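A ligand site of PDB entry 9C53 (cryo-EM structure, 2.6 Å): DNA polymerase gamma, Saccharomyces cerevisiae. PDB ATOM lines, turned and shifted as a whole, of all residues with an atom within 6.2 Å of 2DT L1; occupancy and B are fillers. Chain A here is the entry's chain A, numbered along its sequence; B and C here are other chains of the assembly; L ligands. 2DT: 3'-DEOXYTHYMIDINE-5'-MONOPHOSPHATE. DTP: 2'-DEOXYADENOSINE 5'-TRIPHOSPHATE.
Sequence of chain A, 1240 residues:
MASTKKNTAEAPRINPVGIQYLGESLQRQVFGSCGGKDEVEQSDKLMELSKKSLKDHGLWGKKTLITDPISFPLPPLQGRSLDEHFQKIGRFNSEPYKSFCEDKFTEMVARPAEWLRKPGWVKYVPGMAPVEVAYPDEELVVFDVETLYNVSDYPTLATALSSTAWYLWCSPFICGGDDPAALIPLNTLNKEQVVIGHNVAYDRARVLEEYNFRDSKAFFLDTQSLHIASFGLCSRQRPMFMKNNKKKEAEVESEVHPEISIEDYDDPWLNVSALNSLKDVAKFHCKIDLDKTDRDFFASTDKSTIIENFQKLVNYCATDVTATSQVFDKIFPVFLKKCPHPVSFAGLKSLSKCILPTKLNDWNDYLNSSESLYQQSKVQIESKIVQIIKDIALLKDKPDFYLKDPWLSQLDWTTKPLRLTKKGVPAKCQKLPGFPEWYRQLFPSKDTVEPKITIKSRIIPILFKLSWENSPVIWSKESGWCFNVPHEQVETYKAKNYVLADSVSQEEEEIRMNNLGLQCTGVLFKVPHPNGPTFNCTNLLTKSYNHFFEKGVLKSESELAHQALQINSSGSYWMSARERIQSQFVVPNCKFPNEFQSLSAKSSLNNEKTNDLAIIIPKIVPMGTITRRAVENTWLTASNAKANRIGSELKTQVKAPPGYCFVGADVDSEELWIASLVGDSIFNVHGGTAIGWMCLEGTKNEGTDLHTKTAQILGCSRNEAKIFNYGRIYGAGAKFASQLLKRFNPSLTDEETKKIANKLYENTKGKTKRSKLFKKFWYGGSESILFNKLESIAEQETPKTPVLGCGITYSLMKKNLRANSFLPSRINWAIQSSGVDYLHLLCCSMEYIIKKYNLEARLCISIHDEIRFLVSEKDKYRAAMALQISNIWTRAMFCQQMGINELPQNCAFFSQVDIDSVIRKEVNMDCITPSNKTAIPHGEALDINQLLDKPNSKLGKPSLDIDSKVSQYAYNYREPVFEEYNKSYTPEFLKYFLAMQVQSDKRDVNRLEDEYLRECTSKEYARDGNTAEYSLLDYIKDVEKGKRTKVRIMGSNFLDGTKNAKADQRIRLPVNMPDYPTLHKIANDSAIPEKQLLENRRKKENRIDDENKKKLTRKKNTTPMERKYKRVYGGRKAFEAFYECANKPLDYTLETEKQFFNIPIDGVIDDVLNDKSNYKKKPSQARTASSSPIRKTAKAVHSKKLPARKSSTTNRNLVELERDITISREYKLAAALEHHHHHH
O3' of DG 23 of chain B sits close to OP1 of 2DT L1 (2.9 Å). N1 of DA 19 of chain C lies within hydrogen-bond range of N3 of 2DT L1 (3.2 Å). The guanidinium group (NH2) of Arg 629 sits at hydrogen-bond distance from an oxygen (O2) of 2DT L1. NZ of Lys 921 lies within salt-bridge range of OP1 of 2DT L1, 3.8 Å away. O4 of DT 18 of chain C is in hydrogen-bond range of N6 of DTP L2 (3.3 Å).
His 864 touches 2DT L1 (CD2 to C4', 3.4 Å). Hydrophobic or aromatic side chains that line 2DT L1: His 864. Of the 13 residues printed, 5 come within 4 Å of 2DT L1.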
ATOM      1  N   ARG A 629      10.239   7.813 -11.579  1.00  0.00           N
ATOM      2  CA  ARG A 629      11.657   7.941 -11.292  1.00  0.00           C
ATOM      3  C   ARG A 629      12.263   6.574 -11.014  1.00  0.00           C
ATOM      4  O   ARG A 629      11.563   5.631 -10.649  1.00  0.00           O
ATOM      5  CB  ARG A 629      11.912   8.880 -10.106  1.00  0.00           C
ATOM      6  CG  ARG A 629      11.230  10.233 -10.220  1.00  0.00           C
ATOM      7  CD  ARG A 629      12.126  11.347  -9.694  1.00  0.00           C
ATOM      8  NE  ARG A 629      12.343  11.244  -8.251  1.00  0.00           N
ATOM      9  CZ  ARG A 629      12.902  12.189  -7.517  1.00  0.00           C
ATOM     10  NH1 ARG A 629      13.310  13.335  -8.039  1.00  0.00           N
ATOM     11  NH2 ARG A 629      13.076  11.974  -6.209  1.00  0.00           N
ATOM     12  N   LEU A 636      21.885   4.591  -5.380  1.00  0.00           N
ATOM     13  CA  LEU A 636      21.121   5.827  -5.372  1.00  0.00           C
ATOM     14  C   LEU A 636      20.860   6.331  -3.957  1.00  0.00           C
ATOM     15  O   LEU A 636      20.153   7.335  -3.780  1.00  0.00           O
ATOM     16  CB  LEU A 636      19.786   5.648  -6.106  1.00  0.00           C
ATOM     17  CG  LEU A 636      19.834   5.402  -7.619  1.00  0.00           C
ATOM     18  CD1 LEU A 636      18.483   5.702  -8.240  1.00  0.00           C
ATOM     19  CD2 LEU A 636      20.921   6.232  -8.281  1.00  0.00           C
ATOM     20  N   ALA A 638      23.773   6.172  -1.707  1.00  0.00           N
ATOM     21  CA  ALA A 638      25.125   6.184  -1.148  1.00  0.00           C
ATOM     22  C   ALA A 638      25.466   7.540  -0.540  1.00  0.00           C
ATOM     23  O   ALA A 638      25.100   8.588  -1.073  1.00  0.00           O
ATOM     24  CB  ALA A 638      26.136   5.831  -2.234  1.00  0.00           C
ATOM     25  N   ASN A 640      27.940  10.645   0.799  1.00  0.00           N
ATOM     26  CA  ASN A 640      29.129  11.353   0.377  1.00  0.00           C
ATOM     27  C   ASN A 640      30.213  11.259   1.457  1.00  0.00           C
ATOM     28  O   ASN A 640      29.945  10.900   2.598  1.00  0.00           O
ATOM     29  CB  ASN A 640      28.805  12.820   0.073  1.00  0.00           C
ATOM     30  CG  ASN A 640      27.876  12.973  -1.115  1.00  0.00           C
ATOM     31  OD1 ASN A 640      28.166  12.496  -2.212  1.00  0.00           O
ATOM     32  ND2 ASN A 640      26.747  13.640  -0.899  1.00  0.00           N
ATOM     33  N   LYS A 651      31.501   5.487  -3.214  1.00  0.00           N
ATOM     34  CA  LYS A 651      31.506   5.866  -4.626  1.00  0.00           C
ATOM     35  C   LYS A 651      32.901   6.075  -5.203  1.00  0.00           C
ATOM     36  O   LYS A 651      33.034   6.193  -6.425  1.00  0.00           O
ATOM     37  CB  LYS A 651      30.672   7.137  -4.839  1.00  0.00           C
ATOM     38  CG  LYS A 651      29.192   6.959  -4.580  1.00  0.00           C
ATOM     39  CD  LYS A 651      28.408   8.205  -4.973  1.00  0.00           C
ATOM     40  CE  LYS A 651      28.612   9.330  -3.980  1.00  0.00           C
ATOM     41  NZ  LYS A 651      27.761  10.507  -4.307  1.00  0.00           N
ATOM     42  N   ILE A 863      22.428   9.430 -11.760  1.00  0.00           N
ATOM     43  CA  ILE A 863      21.611   9.769 -10.556  1.00  0.00           C
ATOM     44  C   ILE A 863      20.652  10.876 -11.005  1.00  0.00           C
ATOM     45  O   ILE A 863      20.931  11.493 -12.054  1.00  0.00           O
ATOM     46  CB  ILE A 863      22.484  10.206  -9.364  1.00  0.00           C
ATOM     47  CG1 ILE A 863      23.916   9.673  -9.498  1.00  0.00           C
ATOM     48  CG2 ILE A 863      21.848   9.789  -8.050  1.00  0.00           C
ATOM     49  CD1 ILE A 863      24.313   8.701  -8.422  1.00  0.00           C
ATOM     50  N   HIS A 864      19.570  11.139 -10.283  1.00  0.00           N
ATOM     51  CA  HIS A 864      18.599  12.141 -10.807  1.00  0.00           C
ATOM     52  C   HIS A 864      19.312  13.496 -10.960  1.00  0.00           C
ATOM     53  O   HIS A 864      19.977  13.913  -9.993  1.00  0.00           O
ATOM     54  CB  HIS A 864      17.389  12.297  -9.871  1.00  0.00           C
ATOM     55  CG  HIS A 864      17.210  11.236  -8.838  1.00  0.00           C
ATOM     56  ND1 HIS A 864      16.191  10.310  -8.902  1.00  0.00           N
ATOM     57  CD2 HIS A 864      17.885  10.952  -7.725  1.00  0.00           C
ATOM     58  CE1 HIS A 864      16.260   9.502  -7.863  1.00  0.00           C
ATOM     59  NE2 HIS A 864      17.289   9.868  -7.125  1.00  0.00           N
ATOM     60  N   ASP A 865      19.203  14.128 -12.132  1.00  0.00           N
ATOM     61  CA  ASP A 865      19.780  15.487 -12.387  1.00  0.00           C
ATOM     62  C   ASP A 865      21.309  15.407 -12.602  1.00  0.00           C
ATOM     63  O   ASP A 865      21.906  16.459 -12.874  1.00  0.00           O
ATOM     64  CB  ASP A 865      19.301  16.489 -11.325  1.00  0.00           C
ATOM     65  CG  ASP A 865      20.385  17.220 -10.564  1.00  0.00           C
ATOM     66  OD1 ASP A 865      20.904  16.653  -9.579  1.00  0.00           O
ATOM     67  OD2 ASP A 865      20.700  18.367 -10.940  1.00  0.00           O
ATOM     68  N   LYS A 921      31.762  14.119  -5.672  1.00  0.00           N
ATOM     69  CA  LYS A 921      30.952  15.319  -5.882  1.00  0.00           C
ATOM     70  C   LYS A 921      31.781  16.493  -6.380  1.00  0.00           C
ATOM     71  O   LYS A 921      31.363  17.206  -7.295  1.00  0.00           O
ATOM     72  CB  LYS A 921      30.213  15.684  -4.596  1.00  0.00           C
ATOM     73  CG  LYS A 921      29.245  16.843  -4.756  1.00  0.00           C
ATOM     74  CD  LYS A 921      28.537  17.166  -3.458  1.00  0.00           C
ATOM     75  CE  LYS A 921      27.542  16.077  -3.094  1.00  0.00           C
ATOM     76  NZ  LYS A 921      26.418  16.031  -4.064  1.00  0.00           N
ATOM     77  P    DG B  23      23.459  11.926   2.840  1.00  0.00           P
ATOM     78  OP1  DG B  23      24.819  12.268   2.372  1.00  0.00           O
ATOM     79  OP2  DG B  23      22.696  12.910   3.646  1.00  0.00           O
ATOM     80  O5'  DG B  23      22.587  11.537   1.557  1.00  0.00           O
ATOM     81  C5'  DG B  23      23.073  10.569   0.633  1.00  0.00           C
ATOM     82  C4'  DG B  23      22.019  10.214  -0.400  1.00  0.00           C
ATOM     83  O4'  DG B  23      20.816   9.792   0.255  1.00  0.00           O
ATOM     84  C3'  DG B  23      21.580  11.365  -1.280  1.00  0.00           C
ATOM     85  O3'  DG B  23      22.489  11.523  -2.362  1.00  0.00           O
ATOM     86  C2'  DG B  23      20.202  10.908  -1.757  1.00  0.00           C
ATOM     87  C1'  DG B  23      19.708  10.027  -0.596  1.00  0.00           C
ATOM     88  N9   DG B  23      18.629  10.631   0.178  1.00  0.00           N
ATOM     89  C8   DG B  23      18.704  11.126   1.456  1.00  0.00           C
ATOM     90  N7   DG B  23      17.574  11.604   1.889  1.00  0.00           N
ATOM     91  C5   DG B  23      16.693  11.416   0.846  1.00  0.00           C
ATOM     92  C6   DG B  23      15.312  11.730   0.741  1.00  0.00           C
ATOM     93  O6   DG B  23      14.590  12.267   1.586  1.00  0.00           O
ATOM     94  N1   DG B  23      14.797  11.365  -0.495  1.00  0.00           N
ATOM     95  C2   DG B  23      15.507  10.771  -1.507  1.00  0.00           C
ATOM     96  N2   DG B  23      14.837  10.493  -2.632  1.00  0.00           N
ATOM     97  N3   DG B  23      16.800  10.463  -1.422  1.00  0.00           N
ATOM     98  C4   DG B  23      17.322  10.809  -0.222  1.00  0.00           C
ATOM     99  P    DT C  18       4.078  20.341   7.639  1.00  0.00           P
ATOM    100  OP1  DT C  18       4.606  19.267   8.502  1.00  0.00           O
ATOM    101  OP2  DT C  18       4.047  21.727   8.152  1.00  0.00           O
ATOM    102  O5'  DT C  18       4.881  20.356   6.257  1.00  0.00           O
ATOM    103  C5'  DT C  18       5.097  19.134   5.534  1.00  0.00           C
ATOM    104  C4'  DT C  18       5.250  19.411   4.058  1.00  0.00           C
ATOM    105  O4'  DT C  18       6.446  20.189   3.828  1.00  0.00           O
ATOM    106  C3'  DT C  18       5.439  18.175   3.191  1.00  0.00           C
ATOM    107  O3'  DT C  18       4.176  17.616   2.857  1.00  0.00           O
ATOM    108  C2'  DT C  18       6.134  18.753   1.955  1.00  0.00           C
ATOM    109  C1'  DT C  18       6.987  19.883   2.554  1.00  0.00           C
ATOM    110  N1   DT C  18       8.424  19.517   2.714  1.00  0.00           N
ATOM    111  C2   DT C  18       9.246  19.496   1.608  1.00  0.00           C
ATOM    112  O2   DT C  18       8.858  19.760   0.486  1.00  0.00           O
ATOM    113  N3   DT C  18      10.545  19.160   1.864  1.00  0.00           N
ATOM    114  C4   DT C  18      11.093  18.842   3.087  1.00  0.00           C
ATOM    115  O4   DT C  18      12.276  18.540   3.221  1.00  0.00           O
ATOM    116  C5   DT C  18      10.186  18.882   4.208  1.00  0.00           C
ATOM    117  C7   DT C  18      10.670  18.553   5.587  1.00  0.00           C
ATOM    118  C6   DT C  18       8.905  19.213   3.974  1.00  0.00           C
ATOM    119  P    DA C  19       4.017  16.031   2.669  1.00  0.00           P
ATOM    120  OP1  DA C  19       2.573  15.736   2.549  1.00  0.00           O
ATOM    121  OP2  DA C  19       4.816  15.362   3.714  1.00  0.00           O
ATOM    122  O5'  DA C  19       4.711  15.729   1.259  1.00  0.00           O
ATOM    123  C5'  DA C  19       4.057  16.095   0.047  1.00  0.00           C
ATOM    124  C4'  DA C  19       4.940  15.804  -1.153  1.00  0.00           C
ATOM    125  O4'  DA C  19       6.120  16.624  -1.099  1.00  0.00           O
ATOM    126  C3'  DA C  19       5.474  14.376  -1.230  1.00  0.00           C
ATOM    127  O3'  DA C  19       4.518  13.537  -1.860  1.00  0.00           O
ATOM    128  C2'  DA C  19       6.714  14.547  -2.094  1.00  0.00           C
ATOM    129  C1'  DA C  19       7.200  15.956  -1.724  1.00  0.00           C
ATOM    130  N9   DA C  19       8.347  15.963  -0.826  1.00  0.00           N
ATOM    131  C8   DA C  19       8.374  16.386   0.467  1.00  0.00           C
ATOM    132  N7   DA C  19       9.559  16.272   1.038  1.00  0.00           N
ATOM    133  C5   DA C  19      10.356  15.736   0.035  1.00  0.00           C
ATOM    134  C6   DA C  19      11.710  15.387  -0.001  1.00  0.00           C
ATOM    135  N6   DA C  19      12.543  15.527   1.043  1.00  0.00           N
ATOM    136  N1   DA C  19      12.194  14.882  -1.153  1.00  0.00           N
ATOM    137  C2   DA C  19      11.371  14.742  -2.194  1.00  0.00           C
ATOM    138  N3   DA C  19      10.079  15.040  -2.281  1.00  0.00           N
ATOM    139  C4   DA C  19       9.624  15.543  -1.115  1.00  0.00           C
ATOM    140  P    DC C  20       4.453  11.969  -1.493  1.00  0.00           P
ATOM    141  OP1  DC C  20       3.224  11.423  -2.113  1.00  0.00           O
ATOM    142  OP2  DC C  20       4.670  11.831  -0.039  1.00  0.00           O
ATOM    143  O5'  DC C  20       5.731  11.345  -2.234  1.00  0.00           O
ATOM    144  C5'  DC C  20       5.810  11.345  -3.647  1.00  0.00           C
ATOM    145  C4'  DC C  20       7.178  10.847  -4.106  1.00  0.00           C
ATOM    146  O4'  DC C  20       8.202  11.717  -3.594  1.00  0.00           O
ATOM    147  C3'  DC C  20       7.544   9.467  -3.580  1.00  0.00           C
ATOM    148  O3'  DC C  20       7.031   8.463  -4.452  1.00  0.00           O
ATOM    149  C2'  DC C  20       9.077   9.499  -3.602  1.00  0.00           C
ATOM    150  C1'  DC C  20       9.408  10.993  -3.438  1.00  0.00           C
ATOM    151  N1   DC C  20      10.013  11.356  -2.127  1.00  0.00           N
ATOM    152  C2   DC C  20      11.371  11.074  -1.889  1.00  0.00           C
ATOM    153  O2   DC C  20      12.037  10.517  -2.757  1.00  0.00           O
ATOM    154  N3   DC C  20      11.903  11.420  -0.687  1.00  0.00           N
ATOM    155  C4   DC C  20      11.156  12.028   0.228  1.00  0.00           C
ATOM    156  N4   DC C  20      11.726  12.346   1.395  1.00  0.00           N
ATOM    157  C5   DC C  20       9.776  12.315  -0.001  1.00  0.00           C
ATOM    158  C6   DC C  20       9.260  11.975  -1.177  1.00  0.00           C
HETATM  159  P   2DT L   1      22.364  14.554  -3.438  1.00  0.00           P
HETATM  160  OP1 2DT L   1      23.453  13.728  -4.056  1.00  0.00           O
HETATM  161  OP2 2DT L   1      22.479  14.463  -1.931  1.00  0.00           O
HETATM  162  O5' 2DT L   1      20.912  13.963  -3.912  1.00  0.00           O
HETATM  163  N1  2DT L   1      17.101  13.655  -3.476  1.00  0.00           N
HETATM  164  C6  2DT L   1      18.050  13.835  -2.416  1.00  0.00           C
HETATM  165  C2  2DT L   1      15.700  14.133  -3.323  1.00  0.00           C
HETATM  166  O2  2DT L   1      14.913  13.979  -4.196  1.00  0.00           O
HETATM  167  N3  2DT L   1      15.281  14.801  -2.060  1.00  0.00           N
HETATM  168  C4  2DT L   1      16.247  14.988  -0.984  1.00  0.00           C
HETATM  169  O4  2DT L   1      15.917  15.520   0.018  1.00  0.00           O
HETATM  170  C5  2DT L   1      17.652  14.506  -1.159  1.00  0.00           C
HETATM  171  C5M 2DT L   1      18.662  14.694  -0.035  1.00  0.00           C
HETATM  172  C2' 2DT L   1      17.832  14.089  -5.859  1.00  0.00           C
HETATM  173  C5' 2DT L   1      20.900  12.954  -4.875  1.00  0.00           C
HETATM  174  C4' 2DT L   1      19.643  12.866  -5.497  1.00  0.00           C
HETATM  175  O4' 2DT L   1      18.579  12.310  -4.506  1.00  0.00           O
HETATM  176  C1' 2DT L   1      17.505  12.998  -4.707  1.00  0.00           C
HETATM  177  C3' 2DT L   1      19.113  14.250  -5.876  1.00  0.00           C
HETATM  178  PG  DTP L   2      21.848  22.735  -7.437  1.00  0.00           P
HETATM  179  O1G DTP L   2      22.671  22.524  -6.197  1.00  0.00           O
HETATM  180  O2G DTP L   2      22.009  21.617  -8.431  1.00  0.00           O
HETATM  181  O3G DTP L   2      22.056  24.086  -8.051  1.00  0.00           O
HETATM  182  PB  DTP L   2      19.028  21.822  -7.334  1.00  0.00           P
HETATM  183  O1B DTP L   2      19.213  21.228  -8.681  1.00  0.00           O
HETATM  184  O2B DTP L   2      17.799  22.613  -7.041  1.00  0.00           O
HETATM  185  O3B DTP L   2      20.306  22.719  -6.969  1.00  0.00           O
HETATM  186  PA  DTP L   2      19.719  19.165  -6.256  1.00  0.00           P
HETATM  187  O1A DTP L   2      20.947  19.118  -7.092  1.00  0.00           O
HETATM  188  O2A DTP L   2      19.813  18.673  -4.853  1.00  0.00           O
HETATM  189  O3A DTP L   2      19.158  20.669  -6.233  1.00  0.00           O
HETATM  190  O5' DTP L   2      18.533  18.410  -7.008  1.00  0.00           O
HETATM  191  C5' DTP L   2      17.546  17.705  -6.198  1.00  0.00           C
HETATM  192  C4' DTP L   2      16.215  17.728  -6.902  1.00  0.00           C
HETATM  193  O4' DTP L   2      15.202  17.246  -6.007  1.00  0.00           O
HETATM  194  C3' DTP L   2      15.756  19.118  -7.353  1.00  0.00           C
HETATM  195  O3' DTP L   2      14.928  19.009  -8.503  1.00  0.00           O
HETATM  196  C2' DTP L   2      14.969  19.615  -6.140  1.00  0.00           C
HETATM  197  C1' DTP L   2      14.482  18.349  -5.454  1.00  0.00           C
HETATM  198  N9  DTP L   2      14.712  18.361  -4.006  1.00  0.00           N
HETATM  199  C8  DTP L   2      15.906  18.225  -3.356  1.00  0.00           C
HETATM  200  N7  DTP L   2      15.780  18.282  -2.048  1.00  0.00           N
HETATM  201  C5  DTP L   2      14.426  18.486  -1.835  1.00  0.00           C
HETATM  202  C6  DTP L   2      13.649  18.633  -0.674  1.00  0.00           C
HETATM  203  N6  DTP L   2      14.157  18.611   0.559  1.00  0.00           N
HETATM  204  N1  DTP L   2      12.323  18.809  -0.824  1.00  0.00           N
HETATM  205  C2  DTP L   2      11.816  18.834  -2.067  1.00  0.00           C
HETATM  206  N3  DTP L   2      12.441  18.704  -3.233  1.00  0.00           N
HETATM  207  C4  DTP L   2      13.761  18.526  -3.043  1.00  0.00           C
